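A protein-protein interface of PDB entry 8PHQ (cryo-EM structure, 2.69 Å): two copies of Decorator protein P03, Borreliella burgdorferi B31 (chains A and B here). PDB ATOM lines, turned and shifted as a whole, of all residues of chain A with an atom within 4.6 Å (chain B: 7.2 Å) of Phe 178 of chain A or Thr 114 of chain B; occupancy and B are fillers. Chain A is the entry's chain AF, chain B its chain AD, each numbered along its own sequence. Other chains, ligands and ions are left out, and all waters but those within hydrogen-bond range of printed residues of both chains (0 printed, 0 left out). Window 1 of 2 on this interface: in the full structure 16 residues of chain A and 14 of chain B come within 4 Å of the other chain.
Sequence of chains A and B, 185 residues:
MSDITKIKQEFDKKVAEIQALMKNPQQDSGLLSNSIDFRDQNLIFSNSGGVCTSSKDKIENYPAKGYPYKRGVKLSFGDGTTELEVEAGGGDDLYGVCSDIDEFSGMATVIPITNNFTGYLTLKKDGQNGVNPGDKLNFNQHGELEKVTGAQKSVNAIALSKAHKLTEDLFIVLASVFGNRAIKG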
ATOM      1  N   THR A 114      18.203  16.996 -14.937  1.00  0.00           N
ATOM      2  CA  THR A 114      17.462  16.406 -16.042  1.00  0.00           C
ATOM      3  C   THR A 114      17.901  16.942 -17.398  1.00  0.00           C
ATOM      4  O   THR A 114      17.392  16.478 -18.423  1.00  0.00           O
ATOM      5  CB  THR A 114      15.961  16.642 -15.855  1.00  0.00           C
ATOM      6  OG1 THR A 114      15.682  18.046 -15.926  1.00  0.00           O
ATOM      7  CG2 THR A 114      15.504  16.110 -14.509  1.00  0.00           C
ATOM      8  N   ASN A 115      18.819  17.902 -17.426  1.00  0.00           N
ATOM      9  CA  ASN A 115      19.373  18.443 -18.658  1.00  0.00           C
ATOM     10  C   ASN A 115      20.862  18.136 -18.689  1.00  0.00           C
ATOM     11  O   ASN A 115      21.584  18.457 -17.739  1.00  0.00           O
ATOM     12  CB  ASN A 115      19.126  19.953 -18.750  1.00  0.00           C
ATOM     13  CG  ASN A 115      19.586  20.548 -20.066  1.00  0.00           C
ATOM     14  OD1 ASN A 115      20.057  19.840 -20.956  1.00  0.00           O
ATOM     15  ND2 ASN A 115      19.451  21.861 -20.195  1.00  0.00           N
ATOM     16  N   ASN A 116      21.318  17.510 -19.771  1.00  0.00           N
ATOM     17  CA  ASN A 116      22.715  17.110 -19.864  1.00  0.00           C
ATOM     18  C   ASN A 116      23.619  18.327 -20.026  1.00  0.00           C
ATOM     19  O   ASN A 116      23.239  19.343 -20.613  1.00  0.00           O
ATOM     20  CB  ASN A 116      22.920  16.137 -21.025  1.00  0.00           C
ATOM     21  CG  ASN A 116      22.886  16.821 -22.370  1.00  0.00           C
ATOM     22  OD1 ASN A 116      21.877  17.406 -22.752  1.00  0.00           O
ATOM     23  ND2 ASN A 116      23.991  16.746 -23.100  1.00  0.00           N
ATOM     24  N   ASN A 156      25.299   9.878 -13.733  1.00  0.00           N
ATOM     25  CA  ASN A 156      26.109   9.594 -14.912  1.00  0.00           C
ATOM     26  C   ASN A 156      26.993  10.798 -15.209  1.00  0.00           C
ATOM     27  O   ASN A 156      26.512  11.825 -15.698  1.00  0.00           O
ATOM     28  CB  ASN A 156      25.224   9.260 -16.109  1.00  0.00           C
ATOM     29  CG  ASN A 156      24.939   7.780 -16.229  1.00  0.00           C
ATOM     30  OD1 ASN A 156      25.514   6.967 -15.508  1.00  0.00           O
ATOM     31  ND2 ASN A 156      24.049   7.422 -17.145  1.00  0.00           N
ATOM     32  N   ILE A 158      31.025  11.458 -16.898  1.00  0.00           N
ATOM     33  CA  ILE A 158      32.189  10.861 -17.541  1.00  0.00           C
ATOM     34  C   ILE A 158      33.200  11.958 -17.842  1.00  0.00           C
ATOM     35  O   ILE A 158      32.846  12.994 -18.416  1.00  0.00           O
ATOM     36  CB  ILE A 158      31.806  10.106 -18.827  1.00  0.00           C
ATOM     37  CG1 ILE A 158      30.909   8.913 -18.491  1.00  0.00           C
ATOM     38  CG2 ILE A 158      33.048   9.643 -19.569  1.00  0.00           C
ATOM     39  CD1 ILE A 158      30.548   8.064 -19.687  1.00  0.00           C
ATOM     40  N   SER A 176      31.200  15.352 -18.831  1.00  0.00           N
ATOM     41  CA  SER A 176      29.850  15.292 -19.374  1.00  0.00           C
ATOM     42  C   SER A 176      28.953  14.623 -18.343  1.00  0.00           C
ATOM     43  O   SER A 176      29.195  13.473 -17.958  1.00  0.00           O
ATOM     44  CB  SER A 176      29.818  14.524 -20.694  1.00  0.00           C
ATOM     45  OG  SER A 176      30.568  15.197 -21.688  1.00  0.00           O
ATOM     46  N   VAL A 177      27.933  15.346 -17.896  1.00  0.00           N
ATOM     47  CA  VAL A 177      26.960  14.854 -16.928  1.00  0.00           C
ATOM     48  C   VAL A 177      25.637  14.675 -17.655  1.00  0.00           C
ATOM     49  O   VAL A 177      25.069  15.644 -18.170  1.00  0.00           O
ATOM     50  CB  VAL A 177      26.807  15.817 -15.740  1.00  0.00           C
ATOM     51  CG1 VAL A 177      25.865  15.234 -14.699  1.00  0.00           C
ATOM     52  CG2 VAL A 177      28.167  16.129 -15.134  1.00  0.00           C
ATOM     53  N   PHE A 178      25.145  13.438 -17.698  1.00  0.00           N
ATOM     54  CA  PHE A 178      23.905  13.118 -18.407  1.00  0.00           C
ATOM     55  C   PHE A 178      22.991  12.306 -17.491  1.00  0.00           C
ATOM     56  O   PHE A 178      22.992  11.075 -17.515  1.00  0.00           O
ATOM     57  CB  PHE A 178      24.191  12.391 -19.733  1.00  0.00           C
ATOM     58  CG  PHE A 178      25.225  11.298 -19.636  1.00  0.00           C
ATOM     59  CD1 PHE A 178      26.577  11.598 -19.635  1.00  0.00           C
ATOM     60  CD2 PHE A 178      24.842   9.968 -19.591  1.00  0.00           C
ATOM     61  CE1 PHE A 178      27.523  10.596 -19.558  1.00  0.00           C
ATOM     62  CE2 PHE A 178      25.784   8.963 -19.517  1.00  0.00           C
ATOM     63  CZ  PHE A 178      27.125   9.278 -19.500  1.00  0.00           C
ATOM     64  N   GLY A 179      22.202  13.009 -16.682  1.00  0.00           N
ATOM     65  CA  GLY A 179      21.155  12.383 -15.902  1.00  0.00           C
ATOM     66  C   GLY A 179      21.656  11.523 -14.752  1.00  0.00           C
ATOM     67  O   GLY A 179      22.811  11.578 -14.330  1.00  0.00           O
ATOM     68  N   ASN A 180      20.733  10.713 -14.244  1.00  0.00           N
ATOM     69  CA  ASN A 180      20.986   9.797 -13.141  1.00  0.00           C
ATOM     70  C   ASN A 180      20.835   8.366 -13.639  1.00  0.00           C
ATOM     71  O   ASN A 180      19.834   8.033 -14.281  1.00  0.00           O
ATOM     72  CB  ASN A 180      20.019  10.053 -11.982  1.00  0.00           C
ATOM     73  CG  ASN A 180      20.310  11.348 -11.251  1.00  0.00           C
ATOM     74  OD1 ASN A 180      21.291  12.032 -11.541  1.00  0.00           O
ATOM     75  ND2 ASN A 180      19.453  11.694 -10.299  1.00  0.00           N
ATOM     76  N   LYS B  58      16.917  18.755 -27.546  1.00  0.00           N
ATOM     77  CA  LYS B  58      18.343  19.029 -27.666  1.00  0.00           C
ATOM     78  C   LYS B  58      18.983  18.008 -28.599  1.00  0.00           C
ATOM     79  O   LYS B  58      18.821  16.798 -28.413  1.00  0.00           O
ATOM     80  CB  LYS B  58      19.019  19.000 -26.297  1.00  0.00           C
ATOM     81  CG  LYS B  58      20.507  19.285 -26.340  1.00  0.00           C
ATOM     82  CD  LYS B  58      21.069  19.462 -24.944  1.00  0.00           C
ATOM     83  CE  LYS B  58      22.552  19.780 -24.976  1.00  0.00           C
ATOM     84  NZ  LYS B  58      23.093  20.026 -23.613  1.00  0.00           N
ATOM     85  N   LEU B  75      29.710   6.596 -26.008  1.00  0.00           N
ATOM     86  CA  LEU B  75      30.917   7.367 -26.274  1.00  0.00           C
ATOM     87  C   LEU B  75      32.135   6.454 -26.242  1.00  0.00           C
ATOM     88  O   LEU B  75      32.316   5.677 -25.299  1.00  0.00           O
ATOM     89  CB  LEU B  75      31.076   8.484 -25.243  1.00  0.00           C
ATOM     90  CG  LEU B  75      30.073   9.638 -25.273  1.00  0.00           C
ATOM     91  CD1 LEU B  75      30.448  10.693 -24.244  1.00  0.00           C
ATOM     92  CD2 LEU B  75      30.001  10.250 -26.656  1.00  0.00           C
ATOM     93  N   ASP B  92      24.927  -0.342 -19.624  1.00  0.00           N
ATOM     94  CA  ASP B  92      25.312   0.662 -18.643  1.00  0.00           C
ATOM     95  C   ASP B  92      26.081   1.826 -19.250  1.00  0.00           C
ATOM     96  O   ASP B  92      26.305   2.826 -18.559  1.00  0.00           O
ATOM     97  CB  ASP B  92      26.153   0.017 -17.539  1.00  0.00           C
ATOM     98  CG  ASP B  92      25.570  -1.295 -17.056  1.00  0.00           C
ATOM     99  OD1 ASP B  92      24.419  -1.293 -16.573  1.00  0.00           O
ATOM    100  OD2 ASP B  92      26.262  -2.329 -17.163  1.00  0.00           O
ATOM    101  N   ASP B  93      26.487   1.727 -20.516  1.00  0.00           N
ATOM    102  CA  ASP B  93      27.269   2.765 -21.175  1.00  0.00           C
ATOM    103  C   ASP B  93      26.443   3.573 -22.168  1.00  0.00           C
ATOM    104  O   ASP B  93      27.008   4.298 -22.992  1.00  0.00           O
ATOM    105  CB  ASP B  93      28.480   2.148 -21.876  1.00  0.00           C
ATOM    106  CG  ASP B  93      29.396   1.412 -20.920  1.00  0.00           C
ATOM    107  OD1 ASP B  93      29.102   1.390 -19.708  1.00  0.00           O
ATOM    108  OD2 ASP B  93      30.412   0.852 -21.382  1.00  0.00           O
ATOM    109  N   LEU B  94      25.118   3.467 -22.107  1.00  0.00           N
ATOM    110  CA  LEU B  94      24.269   4.159 -23.066  1.00  0.00           C
ATOM    111  C   LEU B  94      24.335   5.665 -22.850  1.00  0.00           C
ATOM    112  O   LEU B  94      24.136   6.155 -21.734  1.00  0.00           O
ATOM    113  CB  LEU B  94      22.827   3.672 -22.943  1.00  0.00           C
ATOM    114  CG  LEU B  94      21.851   4.246 -23.970  1.00  0.00           C
ATOM    115  CD1 LEU B  94      22.056   3.585 -25.319  1.00  0.00           C
ATOM    116  CD2 LEU B  94      20.420   4.078 -23.497  1.00  0.00           C
ATOM    117  N   TYR B  95      24.612   6.400 -23.925  1.00  0.00           N
ATOM    118  CA  TYR B  95      24.686   7.854 -23.881  1.00  0.00           C
ATOM    119  C   TYR B  95      23.513   8.543 -24.557  1.00  0.00           C
ATOM    120  O   TYR B  95      23.093   9.607 -24.101  1.00  0.00           O
ATOM    121  CB  TYR B  95      25.985   8.342 -24.535  1.00  0.00           C
ATOM    122  CG  TYR B  95      26.080   9.845 -24.646  1.00  0.00           C
ATOM    123  CD1 TYR B  95      26.136  10.642 -23.512  1.00  0.00           C
ATOM    124  CD2 TYR B  95      26.099  10.467 -25.885  1.00  0.00           C
ATOM    125  CE1 TYR B  95      26.218  12.017 -23.610  1.00  0.00           C
ATOM    126  CE2 TYR B  95      26.180  11.839 -25.993  1.00  0.00           C
ATOM    127  CZ  TYR B  95      26.238  12.609 -24.853  1.00  0.00           C
ATOM    128  OH  TYR B  95      26.318  13.978 -24.956  1.00  0.00           O
ATOM    129  N   GLY B  96      22.976   7.963 -25.621  1.00  0.00           N
ATOM    130  CA  GLY B  96      21.871   8.584 -26.319  1.00  0.00           C
ATOM    131  C   GLY B  96      21.375   7.691 -27.429  1.00  0.00           C
ATOM    132  O   GLY B  96      21.689   6.501 -27.474  1.00  0.00           O
ATOM    133  N   ILE B 111      20.386  12.226 -29.987  1.00  0.00           N
ATOM    134  CA  ILE B 111      19.522  12.810 -28.966  1.00  0.00           C
ATOM    135  C   ILE B 111      19.959  12.247 -27.618  1.00  0.00           C
ATOM    136  O   ILE B 111      19.993  11.016 -27.457  1.00  0.00           O
ATOM    137  CB  ILE B 111      18.042  12.508 -29.237  1.00  0.00           C
ATOM    138  CG1 ILE B 111      17.577  13.248 -30.491  1.00  0.00           C
ATOM    139  CG2 ILE B 111      17.192  12.888 -28.037  1.00  0.00           C
ATOM    140  CD1 ILE B 111      16.102  13.112 -30.770  1.00  0.00           C
ATOM    141  N   PRO B 112      20.326  13.088 -26.652  1.00  0.00           N
ATOM    142  CA  PRO B 112      20.777  12.576 -25.354  1.00  0.00           C
ATOM    143  C   PRO B 112      19.677  11.805 -24.642  1.00  0.00           C
ATOM    144  O   PRO B 112      18.485  12.048 -24.841  1.00  0.00           O
ATOM    145  CB  PRO B 112      21.150  13.846 -24.586  1.00  0.00           C
ATOM    146  CG  PRO B 112      21.488  14.831 -25.644  1.00  0.00           C
ATOM    147  CD  PRO B 112      20.544  14.539 -26.774  1.00  0.00           C
ATOM    148  N   ILE B 113      20.099  10.855 -23.804  1.00  0.00           N
ATOM    149  CA  ILE B 113      19.157  10.022 -23.069  1.00  0.00           C
ATOM    150  C   ILE B 113      18.305  10.844 -22.113  1.00  0.00           C
ATOM    151  O   ILE B 113      17.192  10.433 -21.767  1.00  0.00           O
ATOM    152  CB  ILE B 113      19.914   8.899 -22.327  1.00  0.00           C
ATOM    153  CG1 ILE B 113      18.938   7.838 -21.817  1.00  0.00           C
ATOM    154  CG2 ILE B 113      20.743   9.467 -21.185  1.00  0.00           C
ATOM    155  CD1 ILE B 113      18.098   7.213 -22.905  1.00  0.00           C
ATOM    156  N   THR B 114      18.793  12.009 -21.682  1.00  0.00           N
ATOM    157  CA  THR B 114      18.019  12.873 -20.799  1.00  0.00           C
ATOM    158  C   THR B 114      16.829  13.517 -21.497  1.00  0.00           C
ATOM    159  O   THR B 114      15.968  14.083 -20.816  1.00  0.00           O
ATOM    160  CB  THR B 114      18.912  13.965 -20.210  1.00  0.00           C
ATOM    161  OG1 THR B 114      19.480  14.744 -21.268  1.00  0.00           O
ATOM    162  CG2 THR B 114      20.030  13.351 -19.383  1.00  0.00           C
ATOM    163  N   ASN B 115      16.763  13.452 -22.822  1.00  0.00           N
ATOM    164  CA  ASN B 115      15.661  14.009 -23.593  1.00  0.00           C
ATOM    165  C   ASN B 115      14.844  12.863 -24.176  1.00  0.00           C
ATOM    166  O   ASN B 115      15.389  12.001 -24.870  1.00  0.00           O
ATOM    167  CB  ASN B 115      16.188  14.920 -24.704  1.00  0.00           C
ATOM    168  CG  ASN B 115      15.080  15.587 -25.488  1.00  0.00           C
ATOM    169  OD1 ASN B 115      14.317  16.386 -24.949  1.00  0.00           O
ATOM    170  ND2 ASN B 115      14.985  15.262 -26.771  1.00  0.00           N
ATOM    171  N   ASN B 116      13.544  12.855 -23.890  1.00  0.00           N
ATOM    172  CA  ASN B 116      12.696  11.747 -24.312  1.00  0.00           C
ATOM    173  C   ASN B 116      12.529  11.736 -25.827  1.00  0.00           C
ATOM    174  O   ASN B 116      12.596  12.772 -26.493  1.00  0.00           O
ATOM    175  CB  ASN B 116      11.330  11.826 -23.634  1.00  0.00           C
ATOM    176  CG  ASN B 116      10.556  13.064 -24.027  1.00  0.00           C
ATOM    177  OD1 ASN B 116      11.008  14.187 -23.812  1.00  0.00           O
ATOM    178  ND2 ASN B 116       9.376  12.865 -24.604  1.00  0.00           N
ATOM    179  N   PHE B 178      12.113   7.161 -22.534  1.00  0.00           N
ATOM    180  CA  PHE B 178      12.008   8.309 -21.626  1.00  0.00           C
ATOM    181  C   PHE B 178      12.873   8.079 -20.385  1.00  0.00           C
ATOM    182  O   PHE B 178      12.482   7.395 -19.438  1.00  0.00           O
ATOM    183  CB  PHE B 178      10.539   8.602 -21.302  1.00  0.00           C
ATOM    184  CG  PHE B 178       9.803   7.478 -20.616  1.00  0.00           C
ATOM    185  CD1 PHE B 178       9.178   6.495 -21.364  1.00  0.00           C
ATOM    186  CD2 PHE B 178       9.649   7.457 -19.240  1.00  0.00           C
ATOM    187  CE1 PHE B 178       8.481   5.473 -20.750  1.00  0.00           C
ATOM    188  CE2 PHE B 178       8.951   6.437 -18.622  1.00  0.00           C
ATOM    189  CZ  PHE B 178       8.364   5.447 -19.378  1.00  0.00           C
ATOM    190  N   GLY B 179      14.079   8.638 -20.415  1.00  0.00           N
ATOM    191  CA  GLY B 179      14.931   8.686 -19.246  1.00  0.00           C
ATOM    192  C   GLY B 179      15.497   7.338 -18.826  1.00  0.00           C
ATOM    193  O   GLY B 179      15.467   6.345 -19.553  1.00  0.00           O
ATOM    194  N   ASN B 180      16.026   7.332 -17.607  1.00  0.00           N
ATOM    195  CA  ASN B 180      16.612   6.150 -16.997  1.00  0.00           C
ATOM    196  C   ASN B 180      15.726   5.668 -15.858  1.00  0.00           C
ATOM    197  O   ASN B 180      15.266   6.466 -15.035  1.00  0.00           O
ATOM    198  CB  ASN B 180      18.019   6.443 -16.468  1.00  0.00           C
ATOM    199  CG  ASN B 180      18.972   6.884 -17.558  1.00  0.00           C
ATOM    200  OD1 ASN B 180      18.602   6.958 -18.729  1.00  0.00           O
ATOM    201  ND2 ASN B 180      20.210   7.182 -17.180  1.00  0.00           N
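The backbone carbonyl oxygen (O) of Asn 180 of chain A is in hydrogen-bond range of the side-chain amide nitrogen (ND2) of Asn 180 of chain B (3.0 Å). The side-chain amino group (NZ) of Lys 58 of chain B lies within hydrogen-bond range of the side-chain amide oxygen (OD1) of Asn 116 of chain A, 3.0 Å away.
The backbone NH (N) of Phe 178 of chain A is in hydrogen-bond range of the backbone carbonyl oxygen (O) of Asn 156 of chain A (2.9 Å). N of Asn 156 of chain A is in hydrogen-bond range of O of Gly 179 of chain A, 3.1 Å away.
Among the printed residues, pairs that only touch across the chains: Thr 114 of chain A with Thr 114 of chain B (3.4 Å), Gly 179 of chain A with Thr 114 of chain B (3.5 Å), Asn 116 of chain A with Thr 114 of chain B (3.6 Å), Phe 178 of chain A with Thr 114 of chain B (3.7 Å), Asn 156 of chain A with Asn 180 of chain B (3.8 Å), Asn 116 of chain A with Pro 112 of chain B (3.9 Å) and Phe 178 of chain A with Leu 94 of chain B (3.9 Å).
Of the printed residues of chain B, Asn 116 of chain A touches Lys 58, Pro 112 and Thr 114. Of the printed residues of chain B, Phe 178 of chain A touches Leu 94 (3.9 Å) and Thr 114 (3.7 Å). Printed residues of chain A within 4 Å of Pro 112 of chain B: Asn 116 (3.9 Å). Of chain A, only Thr 114 (3.4 Å), Asn 116 (3.6 Å), Phe 178 (3.7 Å) and Gly 179 (3.5 Å) come within 4 Å of Thr 114 of chain B. The nearest printed residue of chain B that does not touch Phe 178 of chain A is Tyr 95 of chain B (4.01 Å). The nearest residue of chain A that does not touch Thr 114 of chain B is Asn 115 of chain A (4.5 Å). The nearest printed residue of chain A that does not touch Asn 180 of chain B is Phe 178 of chain A (4.8 Å).
Of the 16 printed residues of chain B, 5 touch a printed residue of chain A. Printed residues of chain B that touch a printed residue of chain A: Lys 58, Leu 94, Pro 112, Thr 114 and Asn 180. Hydrophobic or aromatic side chains of chain B within 4 Å of the printed part of chain A: Pro 112. Of the 10 printed residues of chain A, 6 touch a printed residue of chain B. Printed residues of chain A that touch a printed residue of chain B: Thr 114, Asn 116, Asn 156, Phe 178, Gly 179 and Asn 180.
Asn 116 of chain A touches Thr 114 of chain B, but with the chains exchanged Thr 114 of chain A does not touch Asn 116 of chain B (7.6 Å). Phe 178 of chain A touches Thr 114 of chain B, but with the chains exchanged Thr 114 of chain A does not touch Phe 178 of chain B (9.7 Å). Gly 179 of chain A touches Thr 114 of chain B, but with the chains exchanged Thr 114 of chain A does not touch Gly 179 of chain B (8.2 Å). Asn 180 of chain A touches its own counterpart, Asn 180 of chain B. Positions printed for both chains: 114, 115, 116, 178, 179 and 180.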
